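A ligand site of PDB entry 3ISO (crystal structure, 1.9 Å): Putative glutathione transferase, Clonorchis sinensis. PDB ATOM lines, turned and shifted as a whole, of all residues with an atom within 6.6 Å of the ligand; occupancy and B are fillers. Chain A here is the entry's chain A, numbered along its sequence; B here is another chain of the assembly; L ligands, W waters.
A nitrogen (N1) of the ligand lies within salt-bridge range of the side-chain carboxylate of Asp 101 of chain B (2.7 Å).
N2 of the ligand is in hydrogen-bond range of O of Leu 55 (2.8 Å).
The indole nitrogen (NE1) of Trp 41 sits at hydrogen-bond distance from an oxygen (O6) of the ligand (2.8 Å).
N of Ser 68 lies within hydrogen-bond range of O2 of the ligand, 2.8 Å away.
An oxygen (O4) of the ligand is in hydrogen-bond range of the indole nitrogen (NE1) of Trp 8 (2.7 Å).
S1 of the ligand sits close to OH of Tyr 7.
O1 of the ligand is in hydrogen-bond range of OG of Ser 68 (2.5 Å).
An oxygen (O6) of the ligand is in salt-bridge range of the side-chain amino group (NZ) of Lys 45 (2.7 Å).
OD1 of Asn 54 sits at hydrogen-bond distance from N3 of the ligand (2.9 Å).
A nitrogen (N1) of the ligand lies close to the side-chain amide nitrogen (NE2) of Gln 67 (2.8 Å).
OE1 of Gln 67 lies close to N of Gly 98 of chain B, 3.5 Å away.
OD2 of Asp 101 of chain B sits close to OE1 of Gln 67.
OH of Tyr 7 sits at hydrogen-bond distance from N of Leu 13.
The side-chain amide nitrogen (NE2) of Gln 67 sits close to the backbone carbonyl oxygen (O) of Gly 97 of chain B.
Leu 13 touches the ligand (CD1 to O1, 3.5 Å).
Pro 56 touches the ligand.
Hydrophobic or aromatic side chains that line the ligand: Trp 8, Leu 13, Trp 41 and Pro 56.
Within 4 Å of the ligand: Tyr 7, Trp 8, Leu 13, Trp 41, Lys 45, Asn 54, Leu 55, Pro 56, Gln 67, Ser 68 and Asp 101 of chain B.
The nearest printed residue that does not touch the ligand is Gly 97 of chain B (4.4 Å).
Water W2 lies within hydrogen-bond range of N of Gln 67, O2 of the ligand, O of Pro 56 and O of Leu 55.
Water W1 lies within hydrogen-bond range of O of Gly 97 of chain B (2.9 Å), N1 of the ligand (3.1 Å), OD1 of Asp 101 of chain B (3.1 Å) and NE2 of Gln 67 (3.3 Å).
Water W4 lies within hydrogen-bond range of NE2 of Gln 67, N of Leu 69 and O1 of the ligand.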
ATOM      1  N   TYR A   7     -11.201 -31.829 -13.801  1.00  0.00           N
ATOM      2  CA  TYR A   7     -12.231 -30.862 -13.422  1.00  0.00           C
ATOM      3  C   TYR A   7     -13.261 -30.759 -14.546  1.00  0.00           C
ATOM      4  O   TYR A   7     -13.011 -31.227 -15.671  1.00  0.00           O
ATOM      5  CB  TYR A   7     -11.537 -29.414 -13.220  1.00  0.00           C
ATOM      6  CG  TYR A   7     -12.478 -28.462 -12.468  1.00  0.00           C
ATOM      7  CD1 TYR A   7     -13.037 -28.814 -11.226  1.00  0.00           C
ATOM      8  CD2 TYR A   7     -12.789 -27.202 -13.015  1.00  0.00           C
ATOM      9  CE1 TYR A   7     -13.878 -27.911 -10.546  1.00  0.00           C
ATOM     10  CE2 TYR A   7     -13.648 -26.316 -12.336  1.00  0.00           C
ATOM     11  CZ  TYR A   7     -14.155 -26.700 -11.122  1.00  0.00           C
ATOM     12  OH  TYR A   7     -14.954 -25.799 -10.458  1.00  0.00           O
ATOM     13  N   TRP A   8     -14.367 -30.070 -14.250  1.00  0.00           N
ATOM     14  CA  TRP A   8     -15.371 -29.680 -15.266  1.00  0.00           C
ATOM     15  C   TRP A   8     -14.676 -28.789 -16.288  1.00  0.00           C
ATOM     16  O   TRP A   8     -13.643 -28.119 -15.988  1.00  0.00           O
ATOM     17  CB  TRP A   8     -16.538 -28.869 -14.628  1.00  0.00           C
ATOM     18  CG  TRP A   8     -17.229 -29.613 -13.513  1.00  0.00           C
ATOM     19  CD1 TRP A   8     -17.232 -29.335 -12.187  1.00  0.00           C
ATOM     20  CD2 TRP A   8     -18.028 -30.810 -13.691  1.00  0.00           C
ATOM     21  NE1 TRP A   8     -18.007 -30.271 -11.504  1.00  0.00           N
ATOM     22  CE2 TRP A   8     -18.474 -31.198 -12.409  1.00  0.00           C
ATOM     23  CE3 TRP A   8     -18.423 -31.554 -14.822  1.00  0.00           C
ATOM     24  CZ2 TRP A   8     -19.307 -32.313 -12.211  1.00  0.00           C
ATOM     25  CZ3 TRP A   8     -19.189 -32.718 -14.648  1.00  0.00           C
ATOM     26  CH2 TRP A   8     -19.652 -33.068 -13.324  1.00  0.00           C
ATOM     27  N   ILE A  10     -14.753 -25.915 -17.295  1.00  0.00           N
ATOM     28  CA  ILE A  10     -15.226 -24.621 -16.949  1.00  0.00           C
ATOM     29  C   ILE A  10     -14.049 -23.912 -16.218  1.00  0.00           C
ATOM     30  O   ILE A  10     -13.038 -24.563 -15.959  1.00  0.00           O
ATOM     31  CB  ILE A  10     -16.390 -24.626 -15.950  1.00  0.00           C
ATOM     32  CG1 ILE A  10     -15.908 -25.112 -14.575  1.00  0.00           C
ATOM     33  CG2 ILE A  10     -17.636 -25.512 -16.467  1.00  0.00           C
ATOM     34  CD1 ILE A  10     -17.135 -25.194 -13.568  1.00  0.00           C
ATOM     35  N   GLY A  12     -14.216 -21.704 -13.140  1.00  0.00           N
ATOM     36  CA  GLY A  12     -14.536 -22.181 -11.765  1.00  0.00           C
ATOM     37  C   GLY A  12     -13.303 -22.207 -10.856  1.00  0.00           C
ATOM     38  O   GLY A  12     -12.447 -21.280 -10.883  1.00  0.00           O
ATOM     39  N   LEU A  13     -13.216 -23.242 -10.037  1.00  0.00           N
ATOM     40  CA  LEU A  13     -12.170 -23.359  -9.052  1.00  0.00           C
ATOM     41  C   LEU A  13     -10.828 -23.777  -9.602  1.00  0.00           C
ATOM     42  O   LEU A  13      -9.807 -23.686  -8.871  1.00  0.00           O
ATOM     43  CB  LEU A  13     -12.543 -24.444  -8.000  1.00  0.00           C
ATOM     44  CG  LEU A  13     -13.802 -24.058  -7.123  1.00  0.00           C
ATOM     45  CD1 LEU A  13     -14.123 -25.259  -6.251  1.00  0.00           C
ATOM     46  CD2 LEU A  13     -13.694 -22.704  -6.281  1.00  0.00           C
ATOM     47  N   TRP A  41     -18.620 -38.516 -14.509  1.00  0.00           N
ATOM     48  CA  TRP A  41     -17.881 -38.154 -13.255  1.00  0.00           C
ATOM     49  C   TRP A  41     -18.387 -39.026 -12.084  1.00  0.00           C
ATOM     50  O   TRP A  41     -17.596 -39.608 -11.307  1.00  0.00           O
ATOM     51  CB  TRP A  41     -18.024 -36.674 -12.937  1.00  0.00           C
ATOM     52  CG  TRP A  41     -17.765 -36.384 -11.438  1.00  0.00           C
ATOM     53  CD1 TRP A  41     -18.667 -35.884 -10.542  1.00  0.00           C
ATOM     54  CD2 TRP A  41     -16.567 -36.693 -10.714  1.00  0.00           C
ATOM     55  NE1 TRP A  41     -18.050 -35.832  -9.253  1.00  0.00           N
ATOM     56  CE2 TRP A  41     -16.746 -36.261  -9.379  1.00  0.00           C
ATOM     57  CE3 TRP A  41     -15.309 -37.186 -11.091  1.00  0.00           C
ATOM     58  CZ2 TRP A  41     -15.745 -36.412  -8.405  1.00  0.00           C
ATOM     59  CZ3 TRP A  41     -14.288 -37.286 -10.141  1.00  0.00           C
ATOM     60  CH2 TRP A  41     -14.527 -36.897  -8.801  1.00  0.00           C
ATOM     61  N   GLN A  42     -19.711 -39.118 -11.962  1.00  0.00           N
ATOM     62  CA  GLN A  42     -20.334 -40.045 -10.958  1.00  0.00           C
ATOM     63  C   GLN A  42     -19.725 -41.456 -11.038  1.00  0.00           C
ATOM     64  O   GLN A  42     -19.488 -42.078  -9.985  1.00  0.00           O
ATOM     65  CB  GLN A  42     -21.853 -40.142 -11.087  1.00  0.00           C
ATOM     66  CG  GLN A  42     -22.630 -38.885 -10.723  1.00  0.00           C
ATOM     67  CD  GLN A  42     -22.227 -38.338  -9.382  1.00  0.00           C
ATOM     68  OE1 GLN A  42     -22.161 -39.095  -8.412  1.00  0.00           O
ATOM     69  NE2 GLN A  42     -21.952 -37.027  -9.300  1.00  0.00           N
ATOM     70  N   LYS A  45     -15.746 -41.154  -9.825  1.00  0.00           N
ATOM     71  CA  LYS A  45     -15.569 -40.469  -8.527  1.00  0.00           C
ATOM     72  C   LYS A  45     -14.914 -41.341  -7.482  1.00  0.00           C
ATOM     73  O   LYS A  45     -13.954 -40.939  -6.790  1.00  0.00           O
ATOM     74  CB  LYS A  45     -16.944 -40.029  -8.035  1.00  0.00           C
ATOM     75  CG  LYS A  45     -16.914 -39.281  -6.751  1.00  0.00           C
ATOM     76  CD  LYS A  45     -18.191 -38.508  -6.517  1.00  0.00           C
ATOM     77  CE  LYS A  45     -18.148 -37.975  -5.029  1.00  0.00           C
ATOM     78  NZ  LYS A  45     -19.186 -36.976  -4.813  1.00  0.00           N
ATOM     79  N   PRO A  53     -13.038 -37.844  -2.298  1.00  0.00           N
ATOM     80  CA  PRO A  53     -13.367 -37.543  -3.741  1.00  0.00           C
ATOM     81  C   PRO A  53     -14.062 -36.247  -3.982  1.00  0.00           C
ATOM     82  O   PRO A  53     -15.023 -35.870  -3.300  1.00  0.00           O
ATOM     83  CB  PRO A  53     -14.341 -38.720  -4.151  1.00  0.00           C
ATOM     84  CG  PRO A  53     -13.879 -39.894  -3.214  1.00  0.00           C
ATOM     85  CD  PRO A  53     -13.452 -39.203  -1.870  1.00  0.00           C
ATOM     86  N   ASN A  54     -13.667 -35.573  -5.045  1.00  0.00           N
ATOM     87  CA  ASN A  54     -14.194 -34.286  -5.288  1.00  0.00           C
ATOM     88  C   ASN A  54     -13.664 -33.789  -6.594  1.00  0.00           C
ATOM     89  O   ASN A  54     -12.800 -34.443  -7.172  1.00  0.00           O
ATOM     90  CB  ASN A  54     -13.857 -33.304  -4.123  1.00  0.00           C
ATOM     91  CG  ASN A  54     -14.997 -32.318  -3.844  1.00  0.00           C
ATOM     92  OD1 ASN A  54     -15.708 -31.890  -4.757  1.00  0.00           O
ATOM     93  ND2 ASN A  54     -15.121 -31.855  -2.574  1.00  0.00           N
ATOM     94  N   LEU A  55     -14.188 -32.690  -7.087  1.00  0.00           N
ATOM     95  CA  LEU A  55     -13.547 -31.992  -8.220  1.00  0.00           C
ATOM     96  C   LEU A  55     -13.244 -30.551  -7.759  1.00  0.00           C
ATOM     97  O   LEU A  55     -14.118 -29.901  -7.221  1.00  0.00           O
ATOM     98  CB  LEU A  55     -14.540 -31.851  -9.409  1.00  0.00           C
ATOM     99  CG  LEU A  55     -14.791 -33.214 -10.138  1.00  0.00           C
ATOM    100  CD1 LEU A  55     -16.059 -33.031 -11.116  1.00  0.00           C
ATOM    101  CD2 LEU A  55     -13.586 -33.735 -10.974  1.00  0.00           C
ATOM    102  N   PRO A  56     -12.031 -30.034  -8.090  1.00  0.00           N
ATOM    103  CA  PRO A  56     -11.020 -30.693  -8.884  1.00  0.00           C
ATOM    104  C   PRO A  56     -10.260 -31.795  -8.197  1.00  0.00           C
ATOM    105  O   PRO A  56     -10.221 -31.822  -6.961  1.00  0.00           O
ATOM    106  CB  PRO A  56      -9.967 -29.539  -9.164  1.00  0.00           C
ATOM    107  CG  PRO A  56     -10.096 -28.707  -7.933  1.00  0.00           C
ATOM    108  CD  PRO A  56     -11.626 -28.636  -7.736  1.00  0.00           C
ATOM    109  N   THR A  66      -7.467 -33.842  -3.467  1.00  0.00           N
ATOM    110  CA  THR A  66      -8.568 -33.009  -3.862  1.00  0.00           C
ATOM    111  C   THR A  66      -8.484 -31.715  -3.046  1.00  0.00           C
ATOM    112  O   THR A  66      -7.537 -31.564  -2.273  1.00  0.00           O
ATOM    113  CB  THR A  66      -9.935 -33.677  -3.631  1.00  0.00           C
ATOM    114  OG1 THR A  66      -9.963 -34.122  -2.271  1.00  0.00           O
ATOM    115  CG2 THR A  66     -10.110 -34.900  -4.625  1.00  0.00           C
ATOM    116  N   GLN A  67      -9.449 -30.806  -3.264  1.00  0.00           N
ATOM    117  CA  GLN A  67      -9.547 -29.431  -2.627  1.00  0.00           C
ATOM    118  C   GLN A  67      -8.664 -28.468  -3.436  1.00  0.00           C
ATOM    119  O   GLN A  67      -7.415 -28.650  -3.479  1.00  0.00           O
ATOM    120  CB  GLN A  67      -9.149 -29.444  -1.158  1.00  0.00           C
ATOM    121  CG  GLN A  67     -10.271 -30.193  -0.291  1.00  0.00           C
ATOM    122  CD  GLN A  67     -11.640 -29.465  -0.307  1.00  0.00           C
ATOM    123  OE1 GLN A  67     -12.761 -30.136  -0.255  1.00  0.00           O
ATOM    124  NE2 GLN A  67     -11.586 -28.120  -0.390  1.00  0.00           N
ATOM    125  N   SER A  68      -9.338 -27.588  -4.177  1.00  0.00           N
ATOM    126  CA  SER A  68      -8.658 -26.650  -5.085  1.00  0.00           C
ATOM    127  C   SER A  68      -7.490 -25.965  -4.388  1.00  0.00           C
ATOM    128  O   SER A  68      -6.440 -25.755  -5.016  1.00  0.00           O
ATOM    129  CB  SER A  68      -9.631 -25.601  -5.663  1.00  0.00           C
ATOM    130  OG  SER A  68     -10.331 -24.883  -4.657  1.00  0.00           O
ATOM    131  N   LEU A  69      -7.708 -25.550  -3.149  1.00  0.00           N
ATOM    132  CA  LEU A  69      -6.644 -24.772  -2.440  1.00  0.00           C
ATOM    133  C   LEU A  69      -5.452 -25.676  -2.096  1.00  0.00           C
ATOM    134  O   LEU A  69      -4.317 -25.244  -2.173  1.00  0.00           O
ATOM    135  CB  LEU A  69      -7.215 -24.052  -1.193  1.00  0.00           C
ATOM    136  CG  LEU A  69      -6.137 -23.130  -0.490  1.00  0.00           C
ATOM    137  CD1 LEU A  69      -5.530 -22.022  -1.423  1.00  0.00           C
ATOM    138  CD2 LEU A  69      -6.786 -22.472   0.783  1.00  0.00           C
ATOM    139  N   ILE A  71      -4.490 -28.285  -3.828  1.00  0.00           N
ATOM    140  CA  ILE A  71      -3.754 -28.554  -5.097  1.00  0.00           C
ATOM    141  C   ILE A  71      -2.905 -27.291  -5.465  1.00  0.00           C
ATOM    142  O   ILE A  71      -1.756 -27.346  -5.773  1.00  0.00           O
ATOM    143  CB  ILE A  71      -4.803 -28.884  -6.239  1.00  0.00           C
ATOM    144  CG1 ILE A  71      -5.490 -30.230  -5.938  1.00  0.00           C
ATOM    145  CG2 ILE A  71      -4.042 -28.954  -7.690  1.00  0.00           C
ATOM    146  CD1 ILE A  71      -6.765 -30.394  -6.764  1.00  0.00           C
ATOM    147  N   TYR A 111     -25.726 -19.037  -9.071  1.00  0.00           N
ATOM    148  CA  TYR A 111     -26.550 -20.213  -9.428  1.00  0.00           C
ATOM    149  C   TYR A 111     -28.063 -19.991  -9.142  1.00  0.00           C
ATOM    150  O   TYR A 111     -28.895 -20.777  -9.622  1.00  0.00           O
ATOM    151  CB  TYR A 111     -26.037 -21.424  -8.703  1.00  0.00           C
ATOM    152  CG  TYR A 111     -24.637 -21.858  -9.212  1.00  0.00           C
ATOM    153  CD1 TYR A 111     -23.495 -21.484  -8.527  1.00  0.00           C
ATOM    154  CD2 TYR A 111     -24.489 -22.613 -10.412  1.00  0.00           C
ATOM    155  CE1 TYR A 111     -22.193 -21.892  -8.988  1.00  0.00           C
ATOM    156  CE2 TYR A 111     -23.195 -22.989 -10.885  1.00  0.00           C
ATOM    157  CZ  TYR A 111     -22.073 -22.611 -10.132  1.00  0.00           C
ATOM    158  OH  TYR A 111     -20.767 -22.980 -10.556  1.00  0.00           O
ATOM    159  N   GLY B  97      -9.534 -28.358   3.779  1.00  0.00           N
ATOM    160  CA  GLY B  97     -10.565 -27.816   2.816  1.00  0.00           C
ATOM    161  C   GLY B  97     -11.867 -28.647   2.927  1.00  0.00           C
ATOM    162  O   GLY B  97     -13.036 -28.124   2.788  1.00  0.00           O
ATOM    163  N   GLY B  98     -11.724 -29.956   3.074  1.00  0.00           N
ATOM    164  CA  GLY B  98     -12.964 -30.794   3.147  1.00  0.00           C
ATOM    165  C   GLY B  98     -13.736 -30.507   4.425  1.00  0.00           C
ATOM    166  O   GLY B  98     -14.977 -30.524   4.449  1.00  0.00           O
ATOM    167  N   VAL B 100     -13.694 -27.555   6.005  1.00  0.00           N
ATOM    168  CA  VAL B 100     -14.308 -26.244   5.865  1.00  0.00           C
ATOM    169  C   VAL B 100     -15.673 -26.445   5.111  1.00  0.00           C
ATOM    170  O   VAL B 100     -16.716 -25.869   5.497  1.00  0.00           O
ATOM    171  CB  VAL B 100     -13.393 -25.282   5.030  1.00  0.00           C
ATOM    172  CG1 VAL B 100     -14.162 -24.037   4.592  1.00  0.00           C
ATOM    173  CG2 VAL B 100     -12.107 -24.897   5.787  1.00  0.00           C
ATOM    174  N   ASP B 101     -15.644 -27.259   4.062  1.00  0.00           N
ATOM    175  CA  ASP B 101     -16.881 -27.630   3.303  1.00  0.00           C
ATOM    176  C   ASP B 101     -17.908 -28.299   4.222  1.00  0.00           C
ATOM    177  O   ASP B 101     -19.098 -27.992   4.129  1.00  0.00           O
ATOM    178  CB  ASP B 101     -16.585 -28.639   2.161  1.00  0.00           C
ATOM    179  CG  ASP B 101     -15.780 -28.044   0.947  1.00  0.00           C
ATOM    180  OD1 ASP B 101     -15.675 -26.841   0.804  1.00  0.00           O
ATOM    181  OD2 ASP B 101     -15.301 -28.830   0.111  1.00  0.00           O
HETATM  182  N1  LIG L   1     -13.945 -26.800  -1.277  1.00  0.00           N
HETATM  183  C1  LIG L   1     -13.919 -27.319  -2.651  1.00  0.00           C
HETATM  184  C2  LIG L   1     -12.610 -27.164  -3.406  1.00  0.00           C
HETATM  185  O1  LIG L   1     -12.242 -25.973  -3.377  1.00  0.00           O
HETATM  186  O2  LIG L   1     -12.163 -27.951  -4.269  1.00  0.00           O
HETATM  187  C3  LIG L   1     -15.174 -27.435  -3.456  1.00  0.00           C
HETATM  188  C4  LIG L   1     -15.099 -28.542  -4.568  1.00  0.00           C
HETATM  189  C5  LIG L   1     -16.488 -28.504  -5.306  1.00  0.00           C
HETATM  190  O3  LIG L   1     -17.469 -27.796  -4.710  1.00  0.00           O
HETATM  191  N2  LIG L   1     -16.654 -29.185  -6.410  1.00  0.00           N
HETATM  192  C6  LIG L   1     -17.874 -29.153  -7.193  1.00  0.00           C
HETATM  193  C7  LIG L   1     -18.064 -30.579  -7.678  1.00  0.00           C
HETATM  194  O4  LIG L   1     -18.531 -30.740  -8.924  1.00  0.00           O
HETATM  195  C8  LIG L   1     -17.429 -28.381  -8.456  1.00  0.00           C
HETATM  196  S1  LIG L   1     -17.122 -26.577  -8.142  1.00  0.00           S
HETATM  197  N3  LIG L   1     -17.704 -31.574  -6.896  1.00  0.00           N
HETATM  198  C9  LIG L   1     -17.810 -32.951  -7.381  1.00  0.00           C
HETATM  199  C10 LIG L   1     -18.631 -33.834  -6.396  1.00  0.00           C
HETATM  200  O5  LIG L   1     -19.039 -33.304  -5.349  1.00  0.00           O
HETATM  201  O6  LIG L   1     -18.723 -35.035  -6.693  1.00  0.00           O
HETATM  202  O   HOH W   1     -12.902 -25.648   1.354  1.00  0.00           O
HETATM  203  O   HOH W   2     -11.810 -30.707  -4.791  1.00  0.00           O
HETATM  204  O   HOH W   3     -11.197 -23.364  -1.411  1.00  0.00           O
HETATM  205  O   HOH W   4      -9.853 -25.860  -1.091  1.00  0.00           O
HETATM  206  O   HOH W   5     -13.728 -23.716  -1.509  1.00  0.00           O
